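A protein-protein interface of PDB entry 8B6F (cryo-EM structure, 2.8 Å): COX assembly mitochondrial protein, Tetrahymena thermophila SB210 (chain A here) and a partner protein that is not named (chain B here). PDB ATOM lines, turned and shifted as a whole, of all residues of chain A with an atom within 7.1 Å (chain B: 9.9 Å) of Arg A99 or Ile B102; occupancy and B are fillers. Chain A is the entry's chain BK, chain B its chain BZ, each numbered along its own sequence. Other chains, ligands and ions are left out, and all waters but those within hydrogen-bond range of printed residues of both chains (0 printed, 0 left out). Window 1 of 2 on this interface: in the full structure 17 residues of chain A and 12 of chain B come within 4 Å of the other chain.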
ATOM      1  N   ASN A  40     -14.401  19.554  13.233  1.00  0.00           N
ATOM      2  CA  ASN A  40     -13.046  19.016  13.286  1.00  0.00           C
ATOM      3  C   ASN A  40     -12.391  19.034  11.912  1.00  0.00           C
ATOM      4  O   ASN A  40     -11.201  19.345  11.788  1.00  0.00           O
ATOM      5  CB  ASN A  40     -13.065  17.594  13.846  1.00  0.00           C
ATOM      6  CG  ASN A  40     -13.501  17.546  15.295  1.00  0.00           C
ATOM      7  OD1 ASN A  40     -14.506  16.922  15.632  1.00  0.00           O
ATOM      8  ND2 ASN A  40     -12.742  18.204  16.163  1.00  0.00           N
ATOM      9  N   SER A  44      -9.062  21.081  11.003  1.00  0.00           N
ATOM     10  CA  SER A  44      -7.861  20.395  10.539  1.00  0.00           C
ATOM     11  C   SER A  44      -7.407  20.922   9.185  1.00  0.00           C
ATOM     12  O   SER A  44      -6.217  20.848   8.859  1.00  0.00           O
ATOM     13  CB  SER A  44      -8.107  18.888  10.469  1.00  0.00           C
ATOM     14  OG  SER A  44      -9.136  18.580   9.545  1.00  0.00           O
ATOM     15  N   HIS A  65       1.669   1.397  11.403  1.00  0.00           N
ATOM     16  CA  HIS A  65       1.095   1.391  12.744  1.00  0.00           C
ATOM     17  C   HIS A  65      -0.249   0.676  12.767  1.00  0.00           C
ATOM     18  O   HIS A  65      -0.533  -0.101  13.685  1.00  0.00           O
ATOM     19  CB  HIS A  65       0.945   2.822  13.256  1.00  0.00           C
ATOM     20  CG  HIS A  65       0.522   2.904  14.688  1.00  0.00           C
ATOM     21  ND1 HIS A  65       1.180   2.238  15.700  1.00  0.00           N
ATOM     22  CD2 HIS A  65      -0.494   3.575  15.279  1.00  0.00           C
ATOM     23  CE1 HIS A  65       0.587   2.494  16.851  1.00  0.00           C
ATOM     24  NE2 HIS A  65      -0.432   3.303  16.624  1.00  0.00           N
ATOM     25  N   HIS A  79      -2.301   2.024  21.626  1.00  0.00           N
ATOM     26  CA  HIS A  79      -1.093   2.359  20.885  1.00  0.00           C
ATOM     27  C   HIS A  79       0.171   1.968  21.634  1.00  0.00           C
ATOM     28  O   HIS A  79       1.212   1.757  21.005  1.00  0.00           O
ATOM     29  CB  HIS A  79      -1.066   3.855  20.574  1.00  0.00           C
ATOM     30  CG  HIS A  79      -2.164   4.300  19.661  1.00  0.00           C
ATOM     31  ND1 HIS A  79      -2.811   3.439  18.800  1.00  0.00           N
ATOM     32  CD2 HIS A  79      -2.732   5.514  19.475  1.00  0.00           C
ATOM     33  CE1 HIS A  79      -3.729   4.104  18.124  1.00  0.00           C
ATOM     34  NE2 HIS A  79      -3.702   5.365  18.513  1.00  0.00           N
ATOM     35  N   TYR A  86       4.134   3.484  16.893  1.00  0.00           N
ATOM     36  CA  TYR A  86       3.360   4.610  17.396  1.00  0.00           C
ATOM     37  C   TYR A  86       4.184   5.888  17.364  1.00  0.00           C
ATOM     38  O   TYR A  86       3.692   6.941  16.942  1.00  0.00           O
ATOM     39  CB  TYR A  86       2.874   4.320  18.816  1.00  0.00           C
ATOM     40  CG  TYR A  86       2.078   5.446  19.432  1.00  0.00           C
ATOM     41  CD1 TYR A  86       1.035   6.047  18.739  1.00  0.00           C
ATOM     42  CD2 TYR A  86       2.354   5.893  20.718  1.00  0.00           C
ATOM     43  CE1 TYR A  86       0.299   7.071  19.300  1.00  0.00           C
ATOM     44  CE2 TYR A  86       1.623   6.916  21.289  1.00  0.00           C
ATOM     45  CZ  TYR A  86       0.596   7.501  20.575  1.00  0.00           C
ATOM     46  OH  TYR A  86      -0.136   8.520  21.136  1.00  0.00           O
ATOM     47  N   TRP A  89       4.544   6.960  13.768  1.00  0.00           N
ATOM     48  CA  TRP A  89       3.289   7.522  13.283  1.00  0.00           C
ATOM     49  C   TRP A  89       3.082   8.935  13.813  1.00  0.00           C
ATOM     50  O   TRP A  89       2.682   9.833  13.064  1.00  0.00           O
ATOM     51  CB  TRP A  89       2.135   6.603  13.683  1.00  0.00           C
ATOM     52  CG  TRP A  89       0.767   7.115  13.364  1.00  0.00           C
ATOM     53  CD1 TRP A  89       0.280   7.443  12.135  1.00  0.00           C
ATOM     54  CD2 TRP A  89      -0.303   7.328  14.291  1.00  0.00           C
ATOM     55  NE1 TRP A  89      -1.026   7.858  12.239  1.00  0.00           N
ATOM     56  CE2 TRP A  89      -1.407   7.797  13.553  1.00  0.00           C
ATOM     57  CE3 TRP A  89      -0.432   7.174  15.674  1.00  0.00           C
ATOM     58  CZ2 TRP A  89      -2.624   8.115  14.152  1.00  0.00           C
ATOM     59  CZ3 TRP A  89      -1.641   7.491  16.267  1.00  0.00           C
ATOM     60  CH2 TRP A  89      -2.722   7.957  15.507  1.00  0.00           C
ATOM     61  N   GLN A  90       3.343   9.151  15.104  1.00  0.00           N
ATOM     62  CA  GLN A  90       3.206  10.491  15.668  1.00  0.00           C
ATOM     63  C   GLN A  90       4.146  11.478  14.989  1.00  0.00           C
ATOM     64  O   GLN A  90       3.747  12.600  14.656  1.00  0.00           O
ATOM     65  CB  GLN A  90       3.478  10.458  17.171  1.00  0.00           C
ATOM     66  CG  GLN A  90       2.411   9.754  17.983  1.00  0.00           C
ATOM     67  CD  GLN A  90       2.559  10.016  19.468  1.00  0.00           C
ATOM     68  OE1 GLN A  90       1.581  10.293  20.160  1.00  0.00           O
ATOM     69  NE2 GLN A  90       3.786   9.922  19.966  1.00  0.00           N
ATOM     70  N   ASP A  94       0.467  14.512  11.028  1.00  0.00           N
ATOM     71  CA  ASP A  94       0.027  15.688  11.757  1.00  0.00           C
ATOM     72  C   ASP A  94      -1.146  15.344  12.671  1.00  0.00           C
ATOM     73  O   ASP A  94      -1.802  14.310  12.528  1.00  0.00           O
ATOM     74  CB  ASP A  94      -0.371  16.795  10.778  1.00  0.00           C
ATOM     75  CG  ASP A  94      -0.592  18.129  11.463  1.00  0.00           C
ATOM     76  OD1 ASP A  94       0.387  18.706  11.977  1.00  0.00           O
ATOM     77  OD2 ASP A  94      -1.747  18.603  11.481  1.00  0.00           O
ATOM     78  N   VAL A  95      -1.412  16.243  13.621  1.00  0.00           N
ATOM     79  CA  VAL A  95      -2.443  15.986  14.622  1.00  0.00           C
ATOM     80  C   VAL A  95      -3.810  15.849  13.965  1.00  0.00           C
ATOM     81  O   VAL A  95      -4.599  14.967  14.322  1.00  0.00           O
ATOM     82  CB  VAL A  95      -2.443  17.088  15.699  1.00  0.00           C
ATOM     83  CG1 VAL A  95      -1.267  16.907  16.635  1.00  0.00           C
ATOM     84  CG2 VAL A  95      -2.412  18.474  15.068  1.00  0.00           C
ATOM     85  N   GLY A  96      -4.118  16.718  13.002  1.00  0.00           N
ATOM     86  CA  GLY A  96      -5.407  16.628  12.334  1.00  0.00           C
ATOM     87  C   GLY A  96      -5.557  15.343  11.545  1.00  0.00           C
ATOM     88  O   GLY A  96      -6.614  14.709  11.567  1.00  0.00           O
ATOM     89  N   ILE A  97      -4.506  14.946  10.828  1.00  0.00           N
ATOM     90  CA  ILE A  97      -4.544  13.692  10.082  1.00  0.00           C
ATOM     91  C   ILE A  97      -4.748  12.519  11.031  1.00  0.00           C
ATOM     92  O   ILE A  97      -5.536  11.607  10.757  1.00  0.00           O
ATOM     93  CB  ILE A  97      -3.263  13.532   9.242  1.00  0.00           C
ATOM     94  CG1 ILE A  97      -3.200  14.627   8.175  1.00  0.00           C
ATOM     95  CG2 ILE A  97      -3.200  12.142   8.609  1.00  0.00           C
ATOM     96  CD1 ILE A  97      -1.886  14.696   7.437  1.00  0.00           C
ATOM     97  N   ARG A  98      -4.043  12.527  12.163  1.00  0.00           N
ATOM     98  CA  ARG A  98      -4.196  11.452  13.137  1.00  0.00           C
ATOM     99  C   ARG A  98      -5.611  11.411  13.699  1.00  0.00           C
ATOM    100  O   ARG A  98      -6.186  10.331  13.869  1.00  0.00           O
ATOM    101  CB  ARG A  98      -3.178  11.618  14.262  1.00  0.00           C
ATOM    102  CG  ARG A  98      -1.740  11.381  13.831  1.00  0.00           C
ATOM    103  CD  ARG A  98      -0.798  11.427  15.018  1.00  0.00           C
ATOM    104  NE  ARG A  98      -0.365  12.787  15.314  1.00  0.00           N
ATOM    105  CZ  ARG A  98       0.197  13.164  16.453  1.00  0.00           C
ATOM    106  NH1 ARG A  98       0.367  12.318  17.455  1.00  0.00           N
ATOM    107  NH2 ARG A  98       0.594  14.424  16.594  1.00  0.00           N
ATOM    108  N   ARG A  99      -6.192  12.576  13.989  1.00  0.00           N
ATOM    109  CA  ARG A  99      -7.557  12.607  14.503  1.00  0.00           C
ATOM    110  C   ARG A  99      -8.526  12.009  13.494  1.00  0.00           C
ATOM    111  O   ARG A  99      -9.385  11.191  13.846  1.00  0.00           O
ATOM    112  CB  ARG A  99      -7.956  14.043  14.840  1.00  0.00           C
ATOM    113  CG  ARG A  99      -9.237  14.149  15.648  1.00  0.00           C
ATOM    114  CD  ARG A  99      -8.978  13.848  17.115  1.00  0.00           C
ATOM    115  NE  ARG A  99     -10.179  13.391  17.806  1.00  0.00           N
ATOM    116  CZ  ARG A  99     -10.526  12.120  17.956  1.00  0.00           C
ATOM    117  NH1 ARG A  99      -9.780  11.137  17.482  1.00  0.00           N
ATOM    118  NH2 ARG A  99     -11.651  11.829  18.601  1.00  0.00           N
ATOM    119  N   TYR A 100      -8.409  12.411  12.228  1.00  0.00           N
ATOM    120  CA  TYR A 100      -9.278  11.858  11.196  1.00  0.00           C
ATOM    121  C   TYR A 100      -9.090  10.352  11.074  1.00  0.00           C
ATOM    122  O   TYR A 100     -10.066   9.604  10.945  1.00  0.00           O
ATOM    123  CB  TYR A 100      -8.999  12.539   9.859  1.00  0.00           C
ATOM    124  CG  TYR A 100      -9.758  11.935   8.704  1.00  0.00           C
ATOM    125  CD1 TYR A 100     -11.032  12.376   8.379  1.00  0.00           C
ATOM    126  CD2 TYR A 100      -9.198  10.925   7.933  1.00  0.00           C
ATOM    127  CE1 TYR A 100     -11.728  11.828   7.325  1.00  0.00           C
ATOM    128  CE2 TYR A 100      -9.887  10.370   6.876  1.00  0.00           C
ATOM    129  CZ  TYR A 100     -11.151  10.826   6.576  1.00  0.00           C
ATOM    130  OH  TYR A 100     -11.843  10.276   5.524  1.00  0.00           O
ATOM    131  N   GLN A 101      -7.839   9.888  11.106  1.00  0.00           N
ATOM    132  CA  GLN A 101      -7.573   8.461  10.978  1.00  0.00           C
ATOM    133  C   GLN A 101      -8.186   7.675  12.130  1.00  0.00           C
ATOM    134  O   GLN A 101      -8.771   6.608  11.918  1.00  0.00           O
ATOM    135  CB  GLN A 101      -6.067   8.216  10.905  1.00  0.00           C
ATOM    136  CG  GLN A 101      -5.429   8.701   9.615  1.00  0.00           C
ATOM    137  CD  GLN A 101      -3.916   8.717   9.682  1.00  0.00           C
ATOM    138  OE1 GLN A 101      -3.330   8.639  10.759  1.00  0.00           O
ATOM    139  NE2 GLN A 101      -3.275   8.816   8.524  1.00  0.00           N
ATOM    140  N   MET A 102      -8.060   8.183  13.357  1.00  0.00           N
ATOM    141  CA  MET A 102      -8.619   7.471  14.502  1.00  0.00           C
ATOM    142  C   MET A 102     -10.140   7.437  14.446  1.00  0.00           C
ATOM    143  O   MET A 102     -10.753   6.408  14.754  1.00  0.00           O
ATOM    144  CB  MET A 102      -8.149   8.118  15.803  1.00  0.00           C
ATOM    145  CG  MET A 102      -6.654   7.986  16.063  1.00  0.00           C
ATOM    146  SD  MET A 102      -6.046   6.288  15.963  1.00  0.00           S
ATOM    147  CE  MET A 102      -7.143   5.452  17.103  1.00  0.00           C
ATOM    148  N   ASP A 103     -10.771   8.546  14.059  1.00  0.00           N
ATOM    149  CA  ASP A 103     -12.224   8.549  13.929  1.00  0.00           C
ATOM    150  C   ASP A 103     -12.676   7.561  12.864  1.00  0.00           C
ATOM    151  O   ASP A 103     -13.650   6.826  13.059  1.00  0.00           O
ATOM    152  CB  ASP A 103     -12.718   9.956  13.596  1.00  0.00           C
ATOM    153  CG  ASP A 103     -12.425  10.950  14.699  1.00  0.00           C
ATOM    154  OD1 ASP A 103     -12.394  10.538  15.878  1.00  0.00           O
ATOM    155  OD2 ASP A 103     -12.228  12.144  14.390  1.00  0.00           O
ATOM    156  N   ASN A 104     -11.981   7.533  11.726  1.00  0.00           N
ATOM    157  CA  ASN A 104     -12.332   6.589  10.671  1.00  0.00           C
ATOM    158  C   ASN A 104     -12.149   5.153  11.143  1.00  0.00           C
ATOM    159  O   ASN A 104     -12.964   4.278  10.829  1.00  0.00           O
ATOM    160  CB  ASN A 104     -11.493   6.865   9.425  1.00  0.00           C
ATOM    161  CG  ASN A 104     -12.045   6.182   8.192  1.00  0.00           C
ATOM    162  OD1 ASN A 104     -11.587   5.108   7.805  1.00  0.00           O
ATOM    163  ND2 ASN A 104     -13.041   6.803   7.568  1.00  0.00           N
ATOM    164  N   ARG A 105     -11.083   4.890  11.904  1.00  0.00           N
ATOM    165  CA  ARG A 105     -10.863   3.548  12.433  1.00  0.00           C
ATOM    166  C   ARG A 105     -11.974   3.140  13.391  1.00  0.00           C
ATOM    167  O   ARG A 105     -12.434   1.994  13.365  1.00  0.00           O
ATOM    168  CB  ARG A 105      -9.508   3.472  13.131  1.00  0.00           C
ATOM    169  CG  ARG A 105      -8.332   3.328  12.181  1.00  0.00           C
ATOM    170  CD  ARG A 105      -7.046   3.057  12.940  1.00  0.00           C
ATOM    171  NE  ARG A 105      -7.144   1.869  13.780  1.00  0.00           N
ATOM    172  CZ  ARG A 105      -6.934   0.630  13.360  1.00  0.00           C
ATOM    173  NH1 ARG A 105      -6.619   0.369  12.102  1.00  0.00           N
ATOM    174  NH2 ARG A 105      -7.041  -0.375  14.224  1.00  0.00           N
ATOM    175  N   GLU A 106     -12.416   4.063  14.245  1.00  0.00           N
ATOM    176  CA  GLU A 106     -13.517   3.753  15.149  1.00  0.00           C
ATOM    177  C   GLU A 106     -14.783   3.420  14.372  1.00  0.00           C
ATOM    178  O   GLU A 106     -15.484   2.455  14.697  1.00  0.00           O
ATOM    179  CB  GLU A 106     -13.759   4.929  16.095  1.00  0.00           C
ATOM    180  CG  GLU A 106     -14.888   4.703  17.085  1.00  0.00           C
ATOM    181  CD  GLU A 106     -15.093   5.891  18.003  1.00  0.00           C
ATOM    182  OE1 GLU A 106     -14.373   6.896  17.838  1.00  0.00           O
ATOM    183  OE2 GLU A 106     -15.973   5.819  18.886  1.00  0.00           O
ATOM    184  N   ARG B  68     -21.309  12.432  13.758  1.00  0.00           N
ATOM    185  CA  ARG B  68     -20.164  12.680  14.627  1.00  0.00           C
ATOM    186  C   ARG B  68     -20.016  14.167  14.917  1.00  0.00           C
ATOM    187  O   ARG B  68     -19.715  14.561  16.049  1.00  0.00           O
ATOM    188  CB  ARG B  68     -18.889  12.129  13.990  1.00  0.00           C
ATOM    189  CG  ARG B  68     -17.699  12.098  14.936  1.00  0.00           C
ATOM    190  CD  ARG B  68     -16.412  11.712  14.221  1.00  0.00           C
ATOM    191  NE  ARG B  68     -16.537  10.449  13.499  1.00  0.00           N
ATOM    192  CZ  ARG B  68     -16.808  10.341  12.205  1.00  0.00           C
ATOM    193  NH1 ARG B  68     -16.993  11.407  11.442  1.00  0.00           N
ATOM    194  NH2 ARG B  68     -16.898   9.131  11.660  1.00  0.00           N
ATOM    195  N   ARG B  72     -20.379  16.039  18.770  1.00  0.00           N
ATOM    196  CA  ARG B  72     -19.324  16.893  19.302  1.00  0.00           C
ATOM    197  C   ARG B  72     -19.732  18.358  19.299  1.00  0.00           C
ATOM    198  O   ARG B  72     -19.326  19.114  20.187  1.00  0.00           O
ATOM    199  CB  ARG B  72     -18.038  16.694  18.504  1.00  0.00           C
ATOM    200  CG  ARG B  72     -17.524  15.269  18.544  1.00  0.00           C
ATOM    201  CD  ARG B  72     -16.245  15.111  17.747  1.00  0.00           C
ATOM    202  NE  ARG B  72     -15.759  13.738  17.784  1.00  0.00           N
ATOM    203  CZ  ARG B  72     -14.662  13.313  17.173  1.00  0.00           C
ATOM    204  NH1 ARG B  72     -13.904  14.132  16.462  1.00  0.00           N
ATOM    205  NH2 ARG B  72     -14.313  12.035  17.281  1.00  0.00           N
ATOM    206  N   GLU B  94     -16.140  11.054  28.166  1.00  0.00           N
ATOM    207  CA  GLU B  94     -15.963  10.074  27.100  1.00  0.00           C
ATOM    208  C   GLU B  94     -15.346  10.713  25.863  1.00  0.00           C
ATOM    209  O   GLU B  94     -14.454  10.132  25.235  1.00  0.00           O
ATOM    210  CB  GLU B  94     -17.305   9.428  26.757  1.00  0.00           C
ATOM    211  CG  GLU B  94     -17.239   8.453  25.589  1.00  0.00           C
ATOM    212  CD  GLU B  94     -18.575   7.797  25.300  1.00  0.00           C
ATOM    213  OE1 GLU B  94     -19.486   7.900  26.148  1.00  0.00           O
ATOM    214  OE2 GLU B  94     -18.714   7.183  24.222  1.00  0.00           O
ATOM    215  N   HIS B  95     -15.808  11.906  25.491  1.00  0.00           N
ATOM    216  CA  HIS B  95     -15.296  12.564  24.297  1.00  0.00           C
ATOM    217  C   HIS B  95     -13.972  13.277  24.529  1.00  0.00           C
ATOM    218  O   HIS B  95     -13.289  13.612  23.556  1.00  0.00           O
ATOM    219  CB  HIS B  95     -16.325  13.562  23.766  1.00  0.00           C
ATOM    220  CG  HIS B  95     -17.389  12.932  22.924  1.00  0.00           C
ATOM    221  ND1 HIS B  95     -18.484  12.292  23.464  1.00  0.00           N
ATOM    222  CD2 HIS B  95     -17.521  12.834  21.580  1.00  0.00           C
ATOM    223  CE1 HIS B  95     -19.247  11.832  22.488  1.00  0.00           C
ATOM    224  NE2 HIS B  95     -18.685  12.146  21.336  1.00  0.00           N
ATOM    225  N   ALA B  96     -13.592  13.520  25.783  1.00  0.00           N
ATOM    226  CA  ALA B  96     -12.355  14.225  26.085  1.00  0.00           C
ATOM    227  C   ALA B  96     -11.228  13.307  26.534  1.00  0.00           C
ATOM    228  O   ALA B  96     -10.073  13.744  26.556  1.00  0.00           O
ATOM    229  CB  ALA B  96     -12.600  15.281  27.169  1.00  0.00           C
ATOM    230  N   VAL B  97     -11.527  12.060  26.893  1.00  0.00           N
ATOM    231  CA  VAL B  97     -10.514  11.149  27.413  1.00  0.00           C
ATOM    232  C   VAL B  97     -10.441   9.909  26.534  1.00  0.00           C
ATOM    233  O   VAL B  97      -9.385   9.589  25.978  1.00  0.00           O
ATOM    234  CB  VAL B  97     -10.810  10.770  28.876  1.00  0.00           C
ATOM    235  CG1 VAL B  97      -9.745   9.824  29.410  1.00  0.00           C
ATOM    236  CG2 VAL B  97     -10.894  12.016  29.738  1.00  0.00           C
ATOM    237  N   GLN B  98     -11.565   9.202  26.405  1.00  0.00           N
ATOM    238  CA  GLN B  98     -11.570   7.963  25.633  1.00  0.00           C
ATOM    239  C   GLN B  98     -11.235   8.223  24.170  1.00  0.00           C
ATOM    240  O   GLN B  98     -10.485   7.459  23.552  1.00  0.00           O
ATOM    241  CB  GLN B  98     -12.928   7.273  25.759  1.00  0.00           C
ATOM    242  CG  GLN B  98     -13.360   7.019  27.194  1.00  0.00           C
ATOM    243  CD  GLN B  98     -12.363   6.179  27.965  1.00  0.00           C
ATOM    244  OE1 GLN B  98     -11.598   5.413  27.381  1.00  0.00           O
ATOM    245  NE2 GLN B  98     -12.361   6.326  29.285  1.00  0.00           N
ATOM    246  N   LYS B  99     -11.777   9.296  23.599  1.00  0.00           N
ATOM    247  CA  LYS B  99     -11.544   9.634  22.202  1.00  0.00           C
ATOM    248  C   LYS B  99     -10.279  10.456  21.995  1.00  0.00           C
ATOM    249  O   LYS B  99      -9.984  10.836  20.858  1.00  0.00           O
ATOM    250  CB  LYS B  99     -12.747  10.389  21.632  1.00  0.00           C
ATOM    251  CG  LYS B  99     -14.013   9.550  21.569  1.00  0.00           C
ATOM    252  CD  LYS B  99     -15.133  10.287  20.855  1.00  0.00           C
ATOM    253  CE  LYS B  99     -16.430   9.497  20.901  1.00  0.00           C
ATOM    254  NZ  LYS B  99     -16.295   8.150  20.282  1.00  0.00           N
ATOM    255  N   ASN B 100      -9.535  10.750  23.060  1.00  0.00           N
ATOM    256  CA  ASN B 100      -8.224  11.386  22.944  1.00  0.00           C
ATOM    257  C   ASN B 100      -7.159  10.315  22.697  1.00  0.00           C
ATOM    258  O   ASN B 100      -6.207  10.140  23.457  1.00  0.00           O
ATOM    259  CB  ASN B 100      -7.922  12.195  24.198  1.00  0.00           C
ATOM    260  CG  ASN B 100      -6.588  12.906  24.124  1.00  0.00           C
ATOM    261  OD1 ASN B 100      -6.124  13.269  23.044  1.00  0.00           O
ATOM    262  ND2 ASN B 100      -5.959  13.102  25.276  1.00  0.00           N
ATOM    263  N   ASN B 101      -7.345   9.585  21.597  1.00  0.00           N
ATOM    264  CA  ASN B 101      -6.526   8.428  21.270  1.00  0.00           C
ATOM    265  C   ASN B 101      -5.495   8.725  20.186  1.00  0.00           C
ATOM    266  O   ASN B 101      -4.937   7.791  19.602  1.00  0.00           O
ATOM    267  CB  ASN B 101      -7.422   7.263  20.846  1.00  0.00           C
ATOM    268  CG  ASN B 101      -6.735   5.919  20.988  1.00  0.00           C
ATOM    269  OD1 ASN B 101      -5.694   5.806  21.634  1.00  0.00           O
ATOM    270  ND2 ASN B 101      -7.323   4.889  20.391  1.00  0.00           N
ATOM    271  N   ILE B 102      -5.238   9.997  19.901  1.00  0.00           N
ATOM    272  CA  ILE B 102      -4.212  10.365  18.933  1.00  0.00           C
ATOM    273  C   ILE B 102      -2.877   9.774  19.374  1.00  0.00           C
ATOM    274  O   ILE B 102      -2.665   9.495  20.553  1.00  0.00           O
ATOM    275  CB  ILE B 102      -4.117  11.898  18.771  1.00  0.00           C
ATOM    276  CG1 ILE B 102      -5.414  12.441  18.166  1.00  0.00           C
ATOM    277  CG2 ILE B 102      -2.916  12.278  17.905  1.00  0.00           C
ATOM    278  CD1 ILE B 102      -5.456  13.952  18.032  1.00  0.00           C
ATOM    279  OXT ILE B 102      -1.976   9.559  18.564  1.00  0.00           O
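Printed residues of chain B within 4 Å of Val A95: Ile B102.
No residue of chain B comes within 4 Å of Gly A96.
Of the printed residues of chain B, Glu A106 touches Lys B99.
Of the printed residues of chain A, Arg B72 touches Asn A40, Arg A99 and Asp A103.
His B95 touches none of the printed residues of chain A.
Asn B100 touches none of the printed residues of chain A.
Ile B102 touches just these residues of chain A: Tyr A86, Trp A89, Gln A90, Val A95, Arg A98 and Arg A99.
The nearest residue of chain A that does not touch Ile B102 is His A79 (4.1 Å).
The nearest printed residue of chain B that does not touch Asp A103 is Lys B99 (5.5 Å).
ND1 of His A65 sits at hydrogen-bond distance from N of Tyr A86, at 3.4 Å.
The side-chain sulfur (SD) of Met A102 lies within hydrogen-bond range of a ring nitrogen (NE2) of His A79 (3.6 Å).
OG of Ser A44 is in hydrogen-bond range of O of Asn A40 (3.1 Å).
OE1 of Gln A101 sits at hydrogen-bond distance from NE1 of Trp A89.
NH2 of Arg A99 is in salt-bridge range of OD1 of Asp A103 (3.1 Å).
The backbone carbonyl oxygen (O) of Glu B94 is in hydrogen-bond range of the backbone NH (N) of Lys B99 (3.2 Å).
Among the printed residues, merely in contact across the chains: Trp A89 with Ile B102 (3.1 Å), Met A102 with Asn B101 (3.3 Å), Arg A99 with Ile B102 (3.6 Å), Asp A103 with Arg B68 (3.9 Å), Val A95 with Ile B102 (3.9 Å) and Gln A90 with Ile B102 (3.97 Å).
Printed residues of chain B that touch a printed residue of chain A: Arg B68, Arg B72, Lys B99, Asn B101 and Ile B102.
Hydrophobic or aromatic side chains of chain A that line the printed part of chain B: His A79, Tyr A86, Trp A89 and Met A102.
Among the printed residues, 14 pairs touch across the chains.
Among the printed residues, Asp or Glu carboxylates within 4 Å of a Lys or Arg side-chain nitrogen of the other chain: Asp A103 with Arg B72 (2.8 Å) and Glu A106 with Lys B99 (2.7 Å).
The guanidinium group (NH2) of Arg A99 lies close to the guanidinium group (NH2) of Arg B72, 3.0 Å away.
OE2 of Glu A106 lies within salt-bridge range of NZ of Lys B99.
The side-chain hydroxyl (OH) of Tyr A86 is in hydrogen-bond range of the chain-end carboxylate (O) of Ile B102.
The backbone carbonyl oxygen (O) of Asn B101 sits at hydrogen-bond distance from a ring nitrogen (NE2) of His A79 (2.9 Å).
The guanidinium group (NH1) of Arg B72 sits at hydrogen-bond distance from the side-chain amide oxygen (OD1) of Asn A40 (3.0 Å).
The guanidinium group (NH2) of Arg A99 is in hydrogen-bond range of the backbone carbonyl oxygen (O) of Lys B99.
NH1 of Arg A98 lies within salt-bridge range of OXT of Ile B102 (3.8 Å).
The side-chain carboxylate (OD1) of Asp A103 lies within salt-bridge range of the guanidinium group (NH2) of Arg B72, at 2.8 Å.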
